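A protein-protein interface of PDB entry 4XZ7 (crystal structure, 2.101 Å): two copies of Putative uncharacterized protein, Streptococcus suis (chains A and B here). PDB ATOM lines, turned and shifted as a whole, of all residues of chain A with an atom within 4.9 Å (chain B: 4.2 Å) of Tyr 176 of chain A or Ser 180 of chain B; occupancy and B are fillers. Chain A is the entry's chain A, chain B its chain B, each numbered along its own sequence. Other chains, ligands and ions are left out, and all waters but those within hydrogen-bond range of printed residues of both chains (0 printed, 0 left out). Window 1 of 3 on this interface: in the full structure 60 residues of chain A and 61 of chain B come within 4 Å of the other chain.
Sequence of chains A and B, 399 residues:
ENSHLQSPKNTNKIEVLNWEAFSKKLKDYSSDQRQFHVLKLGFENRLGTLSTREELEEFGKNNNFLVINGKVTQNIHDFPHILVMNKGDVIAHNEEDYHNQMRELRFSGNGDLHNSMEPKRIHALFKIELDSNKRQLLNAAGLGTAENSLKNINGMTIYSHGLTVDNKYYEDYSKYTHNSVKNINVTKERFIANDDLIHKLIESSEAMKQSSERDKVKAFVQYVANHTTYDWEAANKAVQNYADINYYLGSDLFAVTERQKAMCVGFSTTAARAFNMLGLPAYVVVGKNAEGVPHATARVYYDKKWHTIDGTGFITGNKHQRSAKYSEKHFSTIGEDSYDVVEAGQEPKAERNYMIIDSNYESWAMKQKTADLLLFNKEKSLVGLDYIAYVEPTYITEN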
ATOM      1  N   ASP A 172       2.407 -11.055  18.844  1.00  0.00           N
ATOM      2  CA  ASP A 172       2.758 -12.452  19.046  1.00  0.00           C
ATOM      3  C   ASP A 172       3.468 -13.031  17.827  1.00  0.00           C
ATOM      4  O   ASP A 172       4.460 -13.732  17.964  1.00  0.00           O
ATOM      5  CB  ASP A 172       1.515 -13.272  19.362  1.00  0.00           C
ATOM      6  CG  ASP A 172       0.716 -12.679  20.508  1.00  0.00           C
ATOM      7  OD1 ASP A 172       1.128 -12.851  21.671  1.00  0.00           O
ATOM      8  OD2 ASP A 172      -0.307 -12.023  20.244  1.00  0.00           O
ATOM      9  N   TYR A 173       2.958 -12.743  16.635  1.00  0.00           N
ATOM     10  CA  TYR A 173       3.621 -13.227  15.432  1.00  0.00           C
ATOM     11  C   TYR A 173       4.995 -12.573  15.298  1.00  0.00           C
ATOM     12  O   TYR A 173       5.966 -13.232  14.912  1.00  0.00           O
ATOM     13  CB  TYR A 173       2.792 -12.939  14.177  1.00  0.00           C
ATOM     14  CG  TYR A 173       1.693 -13.933  13.854  1.00  0.00           C
ATOM     15  CD1 TYR A 173       1.978 -15.263  13.580  1.00  0.00           C
ATOM     16  CD2 TYR A 173       0.373 -13.518  13.772  1.00  0.00           C
ATOM     17  CE1 TYR A 173       0.972 -16.156  13.254  1.00  0.00           C
ATOM     18  CE2 TYR A 173      -0.645 -14.394  13.453  1.00  0.00           C
ATOM     19  CZ  TYR A 173      -0.346 -15.701  13.191  1.00  0.00           C
ATOM     20  OH  TYR A 173      -1.370 -16.546  12.869  1.00  0.00           O
ATOM     21  N   SER A 174       5.069 -11.277  15.623  1.00  0.00           N
ATOM     22  CA  SER A 174       6.294 -10.529  15.373  1.00  0.00           C
ATOM     23  C   SER A 174       7.427 -10.977  16.278  1.00  0.00           C
ATOM     24  O   SER A 174       8.596 -10.819  15.930  1.00  0.00           O
ATOM     25  CB  SER A 174       6.052  -9.025  15.513  1.00  0.00           C
ATOM     26  OG  SER A 174       5.231  -8.601  14.431  1.00  0.00           O
ATOM     27  N   LYS A 175       7.098 -11.558  17.427  1.00  0.00           N
ATOM     28  CA  LYS A 175       8.150 -12.183  18.226  1.00  0.00           C
ATOM     29  C   LYS A 175       8.778 -13.376  17.482  1.00  0.00           C
ATOM     30  O   LYS A 175       9.983 -13.653  17.610  1.00  0.00           O
ATOM     31  CB  LYS A 175       7.605 -12.619  19.583  1.00  0.00           C
ATOM     32  CG  LYS A 175       7.272 -11.425  20.477  1.00  0.00           C
ATOM     33  CD  LYS A 175       6.960 -11.859  21.906  1.00  0.00           C
ATOM     34  CE  LYS A 175       5.992 -10.896  22.580  1.00  0.00           C
ATOM     35  NZ  LYS A 175       4.693 -11.579  22.849  1.00  0.00           N
ATOM     36  N   TYR A 176       7.961 -14.080  16.705  1.00  0.00           N
ATOM     37  CA  TYR A 176       8.460 -15.168  15.889  1.00  0.00           C
ATOM     38  C   TYR A 176       9.277 -14.622  14.737  1.00  0.00           C
ATOM     39  O   TYR A 176      10.320 -15.174  14.432  1.00  0.00           O
ATOM     40  CB  TYR A 176       7.314 -16.053  15.370  1.00  0.00           C
ATOM     41  CG  TYR A 176       6.930 -17.125  16.362  1.00  0.00           C
ATOM     42  CD1 TYR A 176       7.568 -18.353  16.357  1.00  0.00           C
ATOM     43  CD2 TYR A 176       5.951 -16.890  17.340  1.00  0.00           C
ATOM     44  CE1 TYR A 176       7.241 -19.342  17.280  1.00  0.00           C
ATOM     45  CE2 TYR A 176       5.611 -17.884  18.278  1.00  0.00           C
ATOM     46  CZ  TYR A 176       6.271 -19.107  18.236  1.00  0.00           C
ATOM     47  OH  TYR A 176       5.961 -20.109  19.130  1.00  0.00           O
ATOM     48  N   THR A 177       8.820 -13.547  14.104  1.00  0.00           N
ATOM     49  CA  THR A 177       9.628 -12.926  13.049  1.00  0.00           C
ATOM     50  C   THR A 177      11.037 -12.605  13.579  1.00  0.00           C
ATOM     51  O   THR A 177      12.070 -13.033  13.010  1.00  0.00           O
ATOM     52  CB  THR A 177       8.971 -11.631  12.525  1.00  0.00           C
ATOM     53  OG1 THR A 177       7.600 -11.897  12.189  1.00  0.00           O
ATOM     54  CG2 THR A 177       9.697 -11.096  11.303  1.00  0.00           C
ATOM     55  N   HIS A 178      11.068 -11.891  14.700  1.00  0.00           N
ATOM     56  CA  HIS A 178      12.334 -11.528  15.332  1.00  0.00           C
ATOM     57  C   HIS A 178      13.201 -12.732  15.692  1.00  0.00           C
ATOM     58  O   HIS A 178      14.400 -12.743  15.393  1.00  0.00           O
ATOM     59  CB  HIS A 178      12.098 -10.707  16.591  1.00  0.00           C
ATOM     60  CG  HIS A 178      13.358 -10.365  17.316  1.00  0.00           C
ATOM     61  ND1 HIS A 178      14.273  -9.456  16.827  1.00  0.00           N
ATOM     62  CD2 HIS A 178      13.860 -10.815  18.493  1.00  0.00           C
ATOM     63  CE1 HIS A 178      15.285  -9.365  17.672  1.00  0.00           C
ATOM     64  NE2 HIS A 178      15.059 -10.176  18.692  1.00  0.00           N
ATOM     65  N   ASN A 179      12.624 -13.726  16.358  1.00  0.00           N
ATOM     66  CA  ASN A 179      13.409 -14.905  16.724  1.00  0.00           C
ATOM     67  C   ASN A 179      13.877 -15.692  15.508  1.00  0.00           C
ATOM     68  O   ASN A 179      14.868 -16.413  15.588  1.00  0.00           O
ATOM     69  CB  ASN A 179      12.625 -15.820  17.670  1.00  0.00           C
ATOM     70  CG  ASN A 179      12.639 -15.300  19.111  1.00  0.00           C
ATOM     71  OD1 ASN A 179      13.552 -14.579  19.507  1.00  0.00           O
ATOM     72  ND2 ASN A 179      11.619 -15.654  19.890  1.00  0.00           N
ATOM     73  N   SER A 180      13.179 -15.541  14.384  1.00  0.00           N
ATOM     74  CA  SER A 180      13.522 -16.279  13.170  1.00  0.00           C
ATOM     75  C   SER A 180      14.662 -15.601  12.409  1.00  0.00           C
ATOM     76  O   SER A 180      15.381 -16.274  11.677  1.00  0.00           O
ATOM     77  CB  SER A 180      12.291 -16.421  12.251  1.00  0.00           C
ATOM     78  OG  SER A 180      11.993 -15.182  11.601  1.00  0.00           O
ATOM     79  N   ILE A 245      10.436 -23.774  16.730  1.00  0.00           N
ATOM     80  CA  ILE A 245      11.556 -22.872  16.504  1.00  0.00           C
ATOM     81  C   ILE A 245      12.562 -22.998  17.638  1.00  0.00           C
ATOM     82  O   ILE A 245      13.759 -22.762  17.466  1.00  0.00           O
ATOM     83  CB  ILE A 245      11.056 -21.401  16.365  1.00  0.00           C
ATOM     84  CG1 ILE A 245      12.172 -20.497  15.856  1.00  0.00           C
ATOM     85  CG2 ILE A 245      10.463 -20.887  17.693  1.00  0.00           C
ATOM     86  CD1 ILE A 245      11.692 -19.134  15.384  1.00  0.00           C
ATOM     87  N   TYR B 176      10.039 -20.135   9.463  1.00  0.00           N
ATOM     88  CA  TYR B 176       9.369 -19.409  10.527  1.00  0.00           C
ATOM     89  C   TYR B 176       9.191 -17.943  10.170  1.00  0.00           C
ATOM     90  O   TYR B 176       8.163 -17.381  10.488  1.00  0.00           O
ATOM     91  CB  TYR B 176      10.113 -19.542  11.847  1.00  0.00           C
ATOM     92  CG  TYR B 176       9.698 -20.783  12.574  1.00  0.00           C
ATOM     93  CD1 TYR B 176       8.599 -20.780  13.418  1.00  0.00           C
ATOM     94  CD2 TYR B 176      10.385 -21.979  12.384  1.00  0.00           C
ATOM     95  CE1 TYR B 176       8.206 -21.923  14.067  1.00  0.00           C
ATOM     96  CE2 TYR B 176      10.001 -23.127  13.041  1.00  0.00           C
ATOM     97  CZ  TYR B 176       8.910 -23.090  13.878  1.00  0.00           C
ATOM     98  OH  TYR B 176       8.523 -24.235  14.533  1.00  0.00           O
ATOM     99  N   THR B 177      10.170 -17.328   9.506  1.00  0.00           N
ATOM    100  CA  THR B 177       9.990 -15.935   9.076  1.00  0.00           C
ATOM    101  C   THR B 177       8.712 -15.822   8.227  1.00  0.00           C
ATOM    102  O   THR B 177       7.800 -14.996   8.506  1.00  0.00           O
ATOM    103  CB  THR B 177      11.195 -15.412   8.263  1.00  0.00           C
ATOM    104  OG1 THR B 177      12.407 -15.612   9.001  1.00  0.00           O
ATOM    105  CG2 THR B 177      11.046 -13.919   8.002  1.00  0.00           C
ATOM    106  N   HIS B 178       8.638 -16.677   7.208  1.00  0.00           N
ATOM    107  CA  HIS B 178       7.465 -16.680   6.336  1.00  0.00           C
ATOM    108  C   HIS B 178       6.145 -16.884   7.085  1.00  0.00           C
ATOM    109  O   HIS B 178       5.202 -16.096   6.911  1.00  0.00           O
ATOM    110  CB  HIS B 178       7.558 -17.752   5.260  1.00  0.00           C
ATOM    111  CG  HIS B 178       6.290 -17.885   4.474  1.00  0.00           C
ATOM    112  ND1 HIS B 178       5.803 -16.866   3.687  1.00  0.00           N
ATOM    113  CD2 HIS B 178       5.381 -18.887   4.398  1.00  0.00           C
ATOM    114  CE1 HIS B 178       4.660 -17.242   3.141  1.00  0.00           C
ATOM    115  NE2 HIS B 178       4.383 -18.466   3.555  1.00  0.00           N
ATOM    116  N   ASN B 179       6.070 -17.926   7.909  1.00  0.00           N
ATOM    117  CA  ASN B 179       4.803 -18.197   8.600  1.00  0.00           C
ATOM    118  C   ASN B 179       4.460 -17.084   9.591  1.00  0.00           C
ATOM    119  O   ASN B 179       3.289 -16.800   9.844  1.00  0.00           O
ATOM    120  CB  ASN B 179       4.837 -19.552   9.313  1.00  0.00           C
ATOM    121  CG  ASN B 179       4.694 -20.736   8.347  1.00  0.00           C
ATOM    122  OD1 ASN B 179       3.873 -20.714   7.423  1.00  0.00           O
ATOM    123  ND2 ASN B 179       5.500 -21.778   8.567  1.00  0.00           N
ATOM    124  N   SER B 180       5.481 -16.430  10.139  1.00  0.00           N
ATOM    125  CA  SER B 180       5.227 -15.353  11.084  1.00  0.00           C
ATOM    126  C   SER B 180       4.725 -14.079  10.403  1.00  0.00           C
ATOM    127  O   SER B 180       4.076 -13.254  11.060  1.00  0.00           O
ATOM    128  CB  SER B 180       6.487 -15.045  11.885  1.00  0.00           C
ATOM    129  OG  SER B 180       7.334 -14.190  11.144  1.00  0.00           O
ATOM    130  N   VAL B 181       5.014 -13.889   9.107  1.00  0.00           N
ATOM    131  CA  VAL B 181       4.550 -12.644   8.461  1.00  0.00           C
ATOM    132  C   VAL B 181       3.354 -12.800   7.511  1.00  0.00           C
ATOM    133  O   VAL B 181       2.737 -11.812   7.146  1.00  0.00           O
ATOM    134  CB  VAL B 181       5.687 -11.908   7.652  1.00  0.00           C
ATOM    135  CG1 VAL B 181       6.829 -11.509   8.560  1.00  0.00           C
ATOM    136  CG2 VAL B 181       6.185 -12.740   6.468  1.00  0.00           C
ATOM    137  N   LYS B 182       3.002 -14.018   7.127  1.00  0.00           N
ATOM    138  CA  LYS B 182       2.000 -14.190   6.067  1.00  0.00           C
ATOM    139  C   LYS B 182       0.584 -13.763   6.492  1.00  0.00           C
ATOM    140  O   LYS B 182      -0.255 -13.443   5.647  1.00  0.00           O
ATOM    141  CB  LYS B 182       1.998 -15.643   5.588  1.00  0.00           C
ATOM    142  CG  LYS B 182       1.534 -16.657   6.638  1.00  0.00           C
ATOM    143  CD  LYS B 182       1.668 -18.102   6.136  1.00  0.00           C
ATOM    144  CE  LYS B 182       0.903 -19.083   7.041  1.00  0.00           C
ATOM    145  NZ  LYS B 182       1.084 -20.501   6.651  1.00  0.00           N
ATOM    146  N   ILE B 184       0.087 -11.230   8.983  1.00  0.00           N
ATOM    147  CA  ILE B 184       0.072  -9.889   9.553  1.00  0.00           C
ATOM    148  C   ILE B 184       0.361  -8.855   8.476  1.00  0.00           C
ATOM    149  O   ILE B 184       0.544  -9.210   7.310  1.00  0.00           O
ATOM    150  CB  ILE B 184       1.072  -9.730  10.708  1.00  0.00           C
ATOM    151  CG1 ILE B 184       2.498 -10.088  10.272  1.00  0.00           C
ATOM    152  CG2 ILE B 184       0.626 -10.557  11.894  1.00  0.00           C
ATOM    153  CD1 ILE B 184       3.561  -9.840  11.368  1.00  0.00           C
ATOM    154  N   ALA B 243       5.119 -22.663  24.091  1.00  0.00           N
ATOM    155  CA  ALA B 243       5.108 -21.639  23.042  1.00  0.00           C
ATOM    156  C   ALA B 243       4.974 -22.288  21.671  1.00  0.00           C
ATOM    157  O   ALA B 243       5.718 -23.222  21.346  1.00  0.00           O
ATOM    158  CB  ALA B 243       6.365 -20.786  23.101  1.00  0.00           C
ATOM    159  N   ASP B 244       4.028 -21.786  20.874  1.00  0.00           N
ATOM    160  CA  ASP B 244       3.688 -22.416  19.603  1.00  0.00           C
ATOM    161  C   ASP B 244       3.019 -21.428  18.639  1.00  0.00           C
ATOM    162  O   ASP B 244       1.927 -20.924  18.905  1.00  0.00           O
ATOM    163  CB  ASP B 244       2.774 -23.616  19.871  1.00  0.00           C
ATOM    164  CG  ASP B 244       2.422 -24.378  18.624  1.00  0.00           C
ATOM    165  OD1 ASP B 244       1.307 -24.954  18.585  1.00  0.00           O
ATOM    166  OD2 ASP B 244       3.248 -24.402  17.689  1.00  0.00           O
ATOM    167  N   ILE B 245       3.684 -21.150  17.519  1.00  0.00           N
ATOM    168  CA  ILE B 245       3.148 -20.262  16.497  1.00  0.00           C
ATOM    169  C   ILE B 245       1.819 -20.837  15.954  1.00  0.00           C
ATOM    170  O   ILE B 245       0.904 -20.090  15.560  1.00  0.00           O
ATOM    171  CB  ILE B 245       4.182 -20.045  15.339  1.00  0.00           C
ATOM    172  CG1 ILE B 245       3.665 -19.011  14.328  1.00  0.00           C
ATOM    173  CG2 ILE B 245       4.459 -21.349  14.600  1.00  0.00           C
ATOM    174  CD1 ILE B 245       4.623 -18.787  13.169  1.00  0.00           C
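N of Asp 244 of chain B is in hydrogen-bond range of OH of Tyr 176 of chain A (3.1 Å). The side-chain hydroxyl of Tyr 176 of chain B is in hydrogen-bond range of the backbone NH of Ile 245 of chain A (2.9 Å). The side-chain hydroxyl (OH) of Tyr 176 of chain A sits at hydrogen-bond distance from the backbone NH (N) of Ile 245 of chain B (3.0 Å). The side-chain hydroxyl of Ser 180 of chain A sits at hydrogen-bond distance from the side-chain hydroxyl of Thr 177 of chain B. OG1 of Thr 177 of chain A is in hydrogen-bond range of OG of Ser 180 of chain B.
The backbone carbonyl oxygen (O) of Thr 177 of chain B lies within hydrogen-bond range of the side-chain hydroxyl (OG) of Ser 180 of chain B (2.8 Å). The backbone carbonyl oxygen of Tyr 173 of chain A is in hydrogen-bond range of the side-chain hydroxyl of Thr 177 of chain A, 3.4 Å away. The backbone carbonyl oxygen (O) of Thr 177 of chain A lies within hydrogen-bond range of the side-chain hydroxyl (OG) of Ser 180 of chain A (2.6 Å). The backbone carbonyl oxygen (O) of Tyr 176 of chain A lies close to the side-chain hydroxyl (OG) of Ser 180 of chain A, at 3.3 Å. O of Tyr 176 of chain B lies close to OG of Ser 180 of chain B (3.4 Å).
CB of Tyr 173 of chain A touches O of Ser 180 of chain B (3.4 Å). Tyr 173 of chain A touches Ile 184 of chain B. Ile 184 of chain B touches Ser 174 of chain A. Tyr 176 of chain A touches Tyr 176 of chain B. CB of Tyr 176 of chain A touches CB of Ser 180 of chain B (3.7 Å). Tyr 176 of chain A touches Ala 243 of chain B. Val 181 of chain B touches Thr 177 of chain A (CG1 to OG1, 3.7 Å). Ser 180 of chain A touches Tyr 176 of chain B (CB to CB, 3.8 Å).
Tyr 176 of chain A touches just these residues of chain B: Tyr 176 (3.9 Å), Ser 180 (3.7 Å), Ala 243 (3.5 Å), Asp 244 (3.1 Å) and Ile 245 (3.0 Å). Printed residues of chain A within 4 Å of Ser 180 of chain B: Tyr 173, Tyr 176 and Thr 177. Of the printed residues of chain B, Thr 177 of chain A touches Ser 180 and Val 181. Of the printed residues of chain B, Ser 174 of chain A touches Ile 184. Of the printed residues of chain A, Asp 244 of chain B touches Tyr 176. Of the printed residues of chain A, Thr 177 of chain B touches Ser 180 (2.7 Å). Printed residues of chain B within 4 Å of Ile 245 of chain A: Tyr 176. The nearest printed residue of chain B that does not touch Tyr 176 of chain A is Thr 177 of chain B (5.4 Å).
Of the 11 printed residues of chain B, 8 touch a printed residue of chain A. Among the printed residues, 13 pairs touch across the chains.
Tyr 176 of chain B touches its own counterpart, Tyr 176 of chain A. Tyr 176 of chain A touches Ser 180 of chain B, and with the chains exchanged Ser 180 of chain A touches Tyr 176 of chain B. Tyr 176 of chain A touches Ile 245 of chain B, and with the chains exchanged Ile 245 of chain A touches Tyr 176 of chain B. Thr 177 of chain A touches Ser 180 of chain B, and with the chains exchanged Ser 180 of chain A touches Thr 177 of chain B.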
